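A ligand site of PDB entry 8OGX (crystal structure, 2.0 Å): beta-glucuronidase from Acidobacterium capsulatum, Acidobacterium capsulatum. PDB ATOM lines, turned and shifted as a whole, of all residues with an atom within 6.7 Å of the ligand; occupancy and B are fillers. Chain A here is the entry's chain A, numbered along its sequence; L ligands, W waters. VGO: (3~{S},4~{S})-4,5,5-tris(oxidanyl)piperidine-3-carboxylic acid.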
ATOM      1  N   SER A  43      -6.081 -15.735 -25.432  1.00  0.00           N
ATOM      2  CA  SER A  43      -6.514 -17.145 -25.473  1.00  0.00           C
ATOM      3  C   SER A  43      -6.602 -17.605 -26.936  1.00  0.00           C
ATOM      4  O   SER A  43      -6.988 -16.773 -27.808  1.00  0.00           O
ATOM      5  CB  SER A  43      -7.807 -17.289 -24.741  1.00  0.00           C
ATOM      6  OG  SER A  43      -8.383 -18.550 -24.984  1.00  0.00           O
ATOM      7  N   TYR A  44      -6.140 -18.824 -27.203  1.00  0.00           N
ATOM      8  CA  TYR A  44      -6.237 -19.531 -28.502  1.00  0.00           C
ATOM      9  C   TYR A  44      -6.847 -20.920 -28.322  1.00  0.00           C
ATOM     10  O   TYR A  44      -6.910 -21.496 -27.210  1.00  0.00           O
ATOM     11  CB  TYR A  44      -4.867 -19.644 -29.185  1.00  0.00           C
ATOM     12  CG  TYR A  44      -4.349 -18.343 -29.743  1.00  0.00           C
ATOM     13  CD1 TYR A  44      -3.875 -17.332 -28.929  1.00  0.00           C
ATOM     14  CD2 TYR A  44      -4.311 -18.135 -31.107  1.00  0.00           C
ATOM     15  CE1 TYR A  44      -3.406 -16.148 -29.445  1.00  0.00           C
ATOM     16  CE2 TYR A  44      -3.814 -16.968 -31.649  1.00  0.00           C
ATOM     17  CZ  TYR A  44      -3.396 -15.955 -30.819  1.00  0.00           C
ATOM     18  OH  TYR A  44      -2.899 -14.825 -31.377  1.00  0.00           O
ATOM     19  N   GLU A  45      -7.305 -21.444 -29.447  1.00  0.00           N
ATOM     20  CA  GLU A  45      -7.832 -22.821 -29.570  1.00  0.00           C
ATOM     21  C   GLU A  45      -6.665 -23.800 -29.515  1.00  0.00           C
ATOM     22  O   GLU A  45      -5.671 -23.569 -30.207  1.00  0.00           O
ATOM     23  CB  GLU A  45      -8.558 -22.952 -30.891  1.00  0.00           C
ATOM     24  CG  GLU A  45      -9.887 -22.218 -30.907  1.00  0.00           C
ATOM     25  CD  GLU A  45     -10.994 -22.732 -30.000  1.00  0.00           C
ATOM     26  OE1 GLU A  45     -10.857 -23.881 -29.449  1.00  0.00           O
ATOM     27  OE2 GLU A  45     -12.027 -21.970 -29.852  1.00  0.00           O
ATOM     28  N   ARG A  76      -2.999 -18.342 -22.935  1.00  0.00           N
ATOM     29  CA  ARG A  76      -3.927 -19.437 -22.583  1.00  0.00           C
ATOM     30  C   ARG A  76      -4.276 -20.205 -23.858  1.00  0.00           C
ATOM     31  O   ARG A  76      -4.618 -19.590 -24.876  1.00  0.00           O
ATOM     32  CB  ARG A  76      -5.175 -18.968 -21.829  1.00  0.00           C
ATOM     33  CG  ARG A  76      -6.133 -20.106 -21.499  1.00  0.00           C
ATOM     34  CD  ARG A  76      -7.253 -20.283 -22.487  1.00  0.00           C
ATOM     35  NE  ARG A  76      -8.261 -21.277 -22.131  1.00  0.00           N
ATOM     36  CZ  ARG A  76      -9.472 -21.322 -22.687  1.00  0.00           C
ATOM     37  NH1 ARG A  76      -9.781 -20.497 -23.685  1.00  0.00           N
ATOM     38  NH2 ARG A  76     -10.324 -22.268 -22.327  1.00  0.00           N
ATOM     39  N   GLY A  78      -6.746 -23.495 -25.042  1.00  0.00           N
ATOM     40  CA  GLY A  78      -7.929 -24.245 -24.576  1.00  0.00           C
ATOM     41  C   GLY A  78      -9.011 -24.225 -25.616  1.00  0.00           C
ATOM     42  O   GLY A  78      -8.696 -24.548 -26.767  1.00  0.00           O
ATOM     43  N   GLY A  79     -10.218 -23.816 -25.202  1.00  0.00           N
ATOM     44  CA  GLY A  79     -11.396 -23.657 -26.071  1.00  0.00           C
ATOM     45  C   GLY A  79     -12.097 -24.991 -26.293  1.00  0.00           C
ATOM     46  O   GLY A  79     -11.632 -26.037 -25.716  1.00  0.00           O
ATOM     47  N   ASN A  80     -13.151 -24.963 -27.096  1.00  0.00           N
ATOM     48  CA  ASN A  80     -13.948 -26.182 -27.410  1.00  0.00           C
ATOM     49  C   ASN A  80     -12.972 -27.197 -28.027  1.00  0.00           C
ATOM     50  O   ASN A  80     -13.185 -28.413 -27.816  1.00  0.00           O
ATOM     51  CB  ASN A  80     -15.157 -25.876 -28.304  1.00  0.00           C
ATOM     52  CG  ASN A  80     -16.172 -24.944 -27.673  1.00  0.00           C
ATOM     53  OD1 ASN A  80     -16.348 -24.916 -26.450  1.00  0.00           O
ATOM     54  ND2 ASN A  80     -16.899 -24.200 -28.510  1.00  0.00           N
ATOM     55  N   THR A  81     -11.916 -26.763 -28.744  1.00  0.00           N
ATOM     56  CA  THR A  81     -11.034 -27.689 -29.496  1.00  0.00           C
ATOM     57  C   THR A  81     -10.134 -28.484 -28.542  1.00  0.00           C
ATOM     58  O   THR A  81      -9.609 -29.511 -28.993  1.00  0.00           O
ATOM     59  CB  THR A  81     -10.159 -27.066 -30.589  1.00  0.00           C
ATOM     60  OG1 THR A  81      -9.236 -26.130 -30.023  1.00  0.00           O
ATOM     61  CG2 THR A  81     -11.008 -26.423 -31.681  1.00  0.00           C
ATOM     62  N   PRO A 104     -11.255 -19.289 -33.783  1.00  0.00           N
ATOM     63  CA  PRO A 104     -12.158 -19.579 -32.678  1.00  0.00           C
ATOM     64  C   PRO A 104     -13.237 -20.551 -33.144  1.00  0.00           C
ATOM     65  O   PRO A 104     -13.829 -20.352 -34.217  1.00  0.00           O
ATOM     66  CB  PRO A 104     -12.719 -18.196 -32.305  1.00  0.00           C
ATOM     67  CG  PRO A 104     -11.630 -17.244 -32.725  1.00  0.00           C
ATOM     68  CD  PRO A 104     -11.082 -17.839 -33.993  1.00  0.00           C
ATOM     69  N   ASP A 105     -13.445 -21.593 -32.330  1.00  0.00           N
ATOM     70  CA  ASP A 105     -14.499 -22.602 -32.556  1.00  0.00           C
ATOM     71  C   ASP A 105     -15.845 -21.862 -32.594  1.00  0.00           C
ATOM     72  O   ASP A 105     -16.096 -21.078 -31.662  1.00  0.00           O
ATOM     73  CB  ASP A 105     -14.500 -23.679 -31.483  1.00  0.00           C
ATOM     74  CG  ASP A 105     -15.405 -24.832 -31.889  1.00  0.00           C
ATOM     75  OD1 ASP A 105     -14.954 -25.690 -32.657  1.00  0.00           O
ATOM     76  OD2 ASP A 105     -16.526 -24.855 -31.426  1.00  0.00           O
ATOM     77  N   LYS A 106     -16.659 -22.090 -33.627  1.00  0.00           N
ATOM     78  CA  LYS A 106     -17.945 -21.366 -33.808  1.00  0.00           C
ATOM     79  C   LYS A 106     -19.062 -22.034 -32.991  1.00  0.00           C
ATOM     80  O   LYS A 106     -20.166 -21.418 -32.882  1.00  0.00           O
ATOM     81  CB  LYS A 106     -18.280 -21.267 -35.292  1.00  0.00           C
ATOM     82  CG  LYS A 106     -17.401 -20.292 -36.054  1.00  0.00           C
ATOM     83  CD  LYS A 106     -17.644 -20.301 -37.544  1.00  0.00           C
ATOM     84  CE  LYS A 106     -16.894 -19.203 -38.276  1.00  0.00           C
ATOM     85  NZ  LYS A 106     -15.554 -19.648 -38.713  1.00  0.00           N
ATOM     86  N   GLY A 107     -18.784 -23.178 -32.367  1.00  0.00           N
ATOM     87  CA  GLY A 107     -19.677 -23.825 -31.386  1.00  0.00           C
ATOM     88  C   GLY A 107     -20.997 -24.251 -31.999  1.00  0.00           C
ATOM     89  O   GLY A 107     -22.009 -24.131 -31.308  1.00  0.00           O
ATOM     90  N   ASN A 172     -12.536 -27.392 -20.832  1.00  0.00           N
ATOM     91  CA  ASN A 172     -13.030 -26.027 -21.151  1.00  0.00           C
ATOM     92  C   ASN A 172     -14.552 -26.052 -21.029  1.00  0.00           C
ATOM     93  O   ASN A 172     -15.156 -26.988 -21.593  1.00  0.00           O
ATOM     94  CB  ASN A 172     -12.629 -25.649 -22.578  1.00  0.00           C
ATOM     95  CG  ASN A 172     -13.376 -24.449 -23.107  1.00  0.00           C
ATOM     96  OD1 ASN A 172     -12.989 -23.307 -22.848  1.00  0.00           O
ATOM     97  ND2 ASN A 172     -14.445 -24.704 -23.849  1.00  0.00           N
ATOM     98  N   GLU A 173     -15.135 -25.095 -20.308  1.00  0.00           N
ATOM     99  CA  GLU A 173     -16.614 -24.938 -20.199  1.00  0.00           C
ATOM    100  C   GLU A 173     -17.256 -26.311 -19.971  1.00  0.00           C
ATOM    101  O   GLU A 173     -18.113 -26.744 -20.747  1.00  0.00           O
ATOM    102  CB  GLU A 173     -17.129 -24.180 -21.424  1.00  0.00           C
ATOM    103  CG  GLU A 173     -16.569 -22.757 -21.474  1.00  0.00           C
ATOM    104  CD  GLU A 173     -16.944 -21.926 -22.685  1.00  0.00           C
ATOM    105  OE1 GLU A 173     -17.279 -22.496 -23.707  1.00  0.00           O
ATOM    106  OE2 GLU A 173     -16.842 -20.683 -22.599  1.00  0.00           O
ATOM    107  N   LEU A 176     -20.837 -26.741 -20.279  1.00  0.00           N
ATOM    108  CA  LEU A 176     -21.477 -26.807 -21.627  1.00  0.00           C
ATOM    109  C   LEU A 176     -21.226 -28.162 -22.306  1.00  0.00           C
ATOM    110  O   LEU A 176     -21.571 -28.272 -23.479  1.00  0.00           O
ATOM    111  CB  LEU A 176     -20.979 -25.659 -22.496  1.00  0.00           C
ATOM    112  CG  LEU A 176     -21.413 -24.267 -22.040  1.00  0.00           C
ATOM    113  CD1 LEU A 176     -21.259 -23.243 -23.165  1.00  0.00           C
ATOM    114  CD2 LEU A 176     -22.855 -24.265 -21.534  1.00  0.00           C
ATOM    115  N   HIS A 241     -14.936 -17.332 -17.683  1.00  0.00           N
ATOM    116  CA  HIS A 241     -15.093 -16.862 -19.074  1.00  0.00           C
ATOM    117  C   HIS A 241     -16.096 -15.719 -19.052  1.00  0.00           C
ATOM    118  O   HIS A 241     -16.871 -15.608 -18.065  1.00  0.00           O
ATOM    119  CB  HIS A 241     -15.513 -17.984 -20.019  1.00  0.00           C
ATOM    120  CG  HIS A 241     -14.463 -19.028 -20.223  1.00  0.00           C
ATOM    121  ND1 HIS A 241     -14.601 -19.971 -21.191  1.00  0.00           N
ATOM    122  CD2 HIS A 241     -13.256 -19.223 -19.653  1.00  0.00           C
ATOM    123  CE1 HIS A 241     -13.561 -20.782 -21.162  1.00  0.00           C
ATOM    124  NE2 HIS A 241     -12.695 -20.318 -20.240  1.00  0.00           N
ATOM    125  N   TYR A 243     -18.459 -13.519 -22.287  1.00  0.00           N
ATOM    126  CA  TYR A 243     -18.841 -12.884 -23.564  1.00  0.00           C
ATOM    127  C   TYR A 243     -19.907 -11.819 -23.286  1.00  0.00           C
ATOM    128  O   TYR A 243     -20.913 -12.131 -22.619  1.00  0.00           O
ATOM    129  CB  TYR A 243     -19.205 -14.004 -24.534  1.00  0.00           C
ATOM    130  CG  TYR A 243     -17.983 -14.772 -24.983  1.00  0.00           C
ATOM    131  CD1 TYR A 243     -17.474 -15.817 -24.247  1.00  0.00           C
ATOM    132  CD2 TYR A 243     -17.230 -14.336 -26.072  1.00  0.00           C
ATOM    133  CE1 TYR A 243     -16.306 -16.478 -24.611  1.00  0.00           C
ATOM    134  CE2 TYR A 243     -16.059 -14.986 -26.464  1.00  0.00           C
ATOM    135  CZ  TYR A 243     -15.613 -16.073 -25.742  1.00  0.00           C
ATOM    136  OH  TYR A 243     -14.470 -16.724 -26.093  1.00  0.00           O
ATOM    137  N   GLU A 287     -10.805 -16.559 -20.613  1.00  0.00           N
ATOM    138  CA  GLU A 287     -11.317 -16.557 -21.995  1.00  0.00           C
ATOM    139  C   GLU A 287     -12.447 -15.528 -22.069  1.00  0.00           C
ATOM    140  O   GLU A 287     -13.431 -15.690 -21.323  1.00  0.00           O
ATOM    141  CB  GLU A 287     -11.845 -17.914 -22.462  1.00  0.00           C
ATOM    142  CG  GLU A 287     -12.003 -17.984 -23.969  1.00  0.00           C
ATOM    143  CD  GLU A 287     -12.874 -19.112 -24.470  1.00  0.00           C
ATOM    144  OE1 GLU A 287     -12.370 -20.270 -24.509  1.00  0.00           O
ATOM    145  OE2 GLU A 287     -14.049 -18.838 -24.783  1.00  0.00           O
ATOM    146  N   CYS A 291     -18.476 -11.134 -28.463  1.00  0.00           N
ATOM    147  CA  CYS A 291     -19.671 -11.919 -28.859  1.00  0.00           C
ATOM    148  C   CYS A 291     -19.301 -13.379 -29.132  1.00  0.00           C
ATOM    149  O   CYS A 291     -18.318 -13.610 -29.843  1.00  0.00           O
ATOM    150  CB  CYS A 291     -20.325 -11.352 -30.106  1.00  0.00           C
ATOM    151  SG  CYS A 291     -21.811 -12.271 -30.592  1.00  0.00           S
ATOM    152  N   TYR A 292     -20.104 -14.322 -28.645  1.00  0.00           N
ATOM    153  CA  TYR A 292     -19.743 -15.773 -28.652  1.00  0.00           C
ATOM    154  C   TYR A 292     -20.061 -16.371 -30.025  1.00  0.00           C
ATOM    155  O   TYR A 292     -20.492 -15.640 -30.946  1.00  0.00           O
ATOM    156  CB  TYR A 292     -20.328 -16.477 -27.432  1.00  0.00           C
ATOM    157  CG  TYR A 292     -21.834 -16.540 -27.314  1.00  0.00           C
ATOM    158  CD1 TYR A 292     -22.573 -17.351 -28.155  1.00  0.00           C
ATOM    159  CD2 TYR A 292     -22.494 -15.890 -26.275  1.00  0.00           C
ATOM    160  CE1 TYR A 292     -23.947 -17.478 -28.018  1.00  0.00           C
ATOM    161  CE2 TYR A 292     -23.862 -16.015 -26.113  1.00  0.00           C
ATOM    162  CZ  TYR A 292     -24.598 -16.792 -27.006  1.00  0.00           C
ATOM    163  OH  TYR A 292     -25.940 -16.941 -26.852  1.00  0.00           O
ATOM    164  N   GLN A 293     -19.800 -17.672 -30.185  1.00  0.00           N
ATOM    165  CA  GLN A 293     -19.926 -18.384 -31.489  1.00  0.00           C
ATOM    166  C   GLN A 293     -19.004 -17.727 -32.528  1.00  0.00           C
ATOM    167  O   GLN A 293     -19.400 -17.664 -33.695  1.00  0.00           O
ATOM    168  CB  GLN A 293     -21.391 -18.417 -31.956  1.00  0.00           C
ATOM    169  CG  GLN A 293     -22.180 -19.605 -31.377  1.00  0.00           C
ATOM    170  CD  GLN A 293     -23.687 -19.511 -31.453  1.00  0.00           C
ATOM    171  OE1 GLN A 293     -24.291 -18.997 -32.411  1.00  0.00           O
ATOM    172  NE2 GLN A 293     -24.330 -20.039 -30.425  1.00  0.00           N
ATOM    173  N   GLY A 294     -17.784 -17.325 -32.133  1.00  0.00           N
ATOM    174  CA  GLY A 294     -16.730 -16.805 -33.033  1.00  0.00           C
ATOM    175  C   GLY A 294     -16.826 -15.301 -33.292  1.00  0.00           C
ATOM    176  O   GLY A 294     -15.977 -14.757 -34.049  1.00  0.00           O
ATOM    177  N   GLY A 295     -17.824 -14.631 -32.741  1.00  0.00           N
ATOM    178  CA  GLY A 295     -17.980 -13.183 -32.901  1.00  0.00           C
ATOM    179  C   GLY A 295     -18.977 -12.839 -33.975  1.00  0.00           C
ATOM    180  O   GLY A 295     -19.508 -13.743 -34.627  1.00  0.00           O
ATOM    181  N   HIS A 327      -9.856 -14.106 -26.436  1.00  0.00           N
ATOM    182  CA  HIS A 327      -9.833 -15.269 -27.340  1.00  0.00           C
ATOM    183  C   HIS A 327      -9.690 -14.764 -28.771  1.00  0.00           C
ATOM    184  O   HIS A 327     -10.138 -13.627 -29.076  1.00  0.00           O
ATOM    185  CB  HIS A 327     -11.069 -16.139 -27.097  1.00  0.00           C
ATOM    186  CG  HIS A 327     -10.894 -17.508 -27.626  1.00  0.00           C
ATOM    187  ND1 HIS A 327      -9.897 -18.356 -27.157  1.00  0.00           N
ATOM    188  CD2 HIS A 327     -11.621 -18.199 -28.534  1.00  0.00           C
ATOM    189  CE1 HIS A 327      -9.980 -19.492 -27.787  1.00  0.00           C
ATOM    190  NE2 HIS A 327     -11.051 -19.434 -28.644  1.00  0.00           N
ATOM    191  N   TYR A 334     -13.504 -11.720 -33.778  1.00  0.00           N
ATOM    192  CA  TYR A 334     -13.101 -10.988 -32.545  1.00  0.00           C
ATOM    193  C   TYR A 334     -11.601 -11.081 -32.261  1.00  0.00           C
ATOM    194  O   TYR A 334     -11.170 -10.554 -31.215  1.00  0.00           O
ATOM    195  CB  TYR A 334     -13.929 -11.417 -31.329  1.00  0.00           C
ATOM    196  CG  TYR A 334     -13.989 -12.885 -30.983  1.00  0.00           C
ATOM    197  CD1 TYR A 334     -12.825 -13.619 -30.742  1.00  0.00           C
ATOM    198  CD2 TYR A 334     -15.211 -13.509 -30.762  1.00  0.00           C
ATOM    199  CE1 TYR A 334     -12.892 -14.955 -30.371  1.00  0.00           C
ATOM    200  CE2 TYR A 334     -15.291 -14.828 -30.385  1.00  0.00           C
ATOM    201  CZ  TYR A 334     -14.118 -15.544 -30.157  1.00  0.00           C
ATOM    202  OH  TYR A 334     -14.230 -16.859 -29.782  1.00  0.00           O
HETATM  203  C4  VGO L   1     -15.156 -21.824 -26.269  1.00  0.00           C
HETATM  204  C5  VGO L   1     -14.445 -21.398 -27.575  1.00  0.00           C
HETATM  205  C6  VGO L   1     -15.374 -20.574 -28.509  1.00  0.00           C
HETATM  206  N1  VGO L   1     -15.803 -20.690 -25.587  1.00  0.00           N
HETATM  207  C3  VGO L   1     -16.717 -19.950 -26.468  1.00  0.00           C
HETATM  208  O1  VGO L   1     -18.311 -19.086 -28.486  1.00  0.00           O
HETATM  209  C1  VGO L   1     -17.116 -18.737 -28.644  1.00  0.00           C
HETATM  210  O2  VGO L   1     -16.734 -17.893 -29.494  1.00  0.00           O
HETATM  211  C2  VGO L   1     -16.056 -19.435 -27.751  1.00  0.00           C
HETATM  212  O3  VGO L   1     -13.453 -20.475 -27.206  1.00  0.00           O
HETATM  213  O4  VGO L   1     -13.824 -22.475 -28.224  1.00  0.00           O
HETATM  214  O5  VGO L   1     -16.380 -21.383 -29.136  1.00  0.00           O
HETATM  215  O   HOH W   1     -19.140 -21.806 -28.464  1.00  0.00           O
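Water W1 bridges an oxygen (O1) of the ligand (2.8 Å) and the side-chain amide nitrogen of Asn 80 (3.3 Å).
A nitrogen (N1) of the ligand lies within salt-bridge range of the side-chain carboxylate of Glu 287, at 2.7 Å.
O4 of the ligand is in hydrogen-bond range of N of Asn 80 (2.8 Å).
An oxygen (O2) of the ligand lies within hydrogen-bond range of the backbone NH (N) of Gly 294 (2.9 Å).
The side-chain carboxylate of Glu 173 is in salt-bridge range of a nitrogen (N1) of the ligand (3.0 Å).
The side-chain amide nitrogen of Asn 80 sits at hydrogen-bond distance from an oxygen (O5) of the ligand (2.9 Å).
An oxygen (O2) of the ligand is in hydrogen-bond range of the side-chain hydroxyl of Tyr 334, at 2.7 Å.
An oxygen (O4) of the ligand is in hydrogen-bond range of the side-chain carboxylate (OE2) of Glu 45 (2.5 Å).
The backbone NH (N) of Gln 293 sits at hydrogen-bond distance from an oxygen (O1) of the ligand (2.7 Å).
The backbone carbonyl oxygen (O) of Asp 105 is in hydrogen-bond range of an oxygen (O5) of the ligand, at 2.6 Å.
A ring nitrogen (NE2) of His 327 lies within hydrogen-bond range of an oxygen (O3) of the ligand, 3.0 Å away.
CA of Gly 79 touches O4 of the ligand, 3.5 Å away.
ND2 of Asn 172 touches C4 of the ligand, at 3.8 Å.
Tyr 243 touches the ligand (OH to C2, 3.6 Å).
CB of Tyr 292 touches O1 of the ligand, at 3.5 Å.
Hydrophobic or aromatic side chains within 4 Å of the ligand: Tyr 243, Tyr 292, His 327 and Tyr 334.
13 residues have an atom within 4 Å of the ligand: Glu 45, Gly 79, Asn 80, Asp 105, Asn 172, Glu 173, Tyr 243, Glu 287, Tyr 292, Gln 293, Gly 294, His 327 and Tyr 334.
The side-chain carboxylate (OD2) of Asp 105 lies within hydrogen-bond range of the side-chain amide nitrogen (ND2) of Asn 80, 3.0 Å away.
ND1 of His 241 is in hydrogen-bond range of OE2 of Glu 173 (2.7 Å).
The side-chain amide oxygen (OD1) of Asn 80 lies within hydrogen-bond range of the side-chain amide nitrogen (ND2) of Asn 172, at 3.2 Å.
A ring nitrogen (ND1) of His 327 is in hydrogen-bond range of the side-chain hydroxyl (OG) of Ser 43.
OH of Tyr 243 lies within hydrogen-bond range of OE2 of Glu 287 (2.5 Å).
OD2 of Asp 105 sits at hydrogen-bond distance from N of Gly 107.
OG1 of Thr 81 sits at hydrogen-bond distance from OE1 of Glu 45 (2.8 Å).
OD1 of Asn 172 is in hydrogen-bond range of NH2 of Arg 76, 2.9 Å away.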
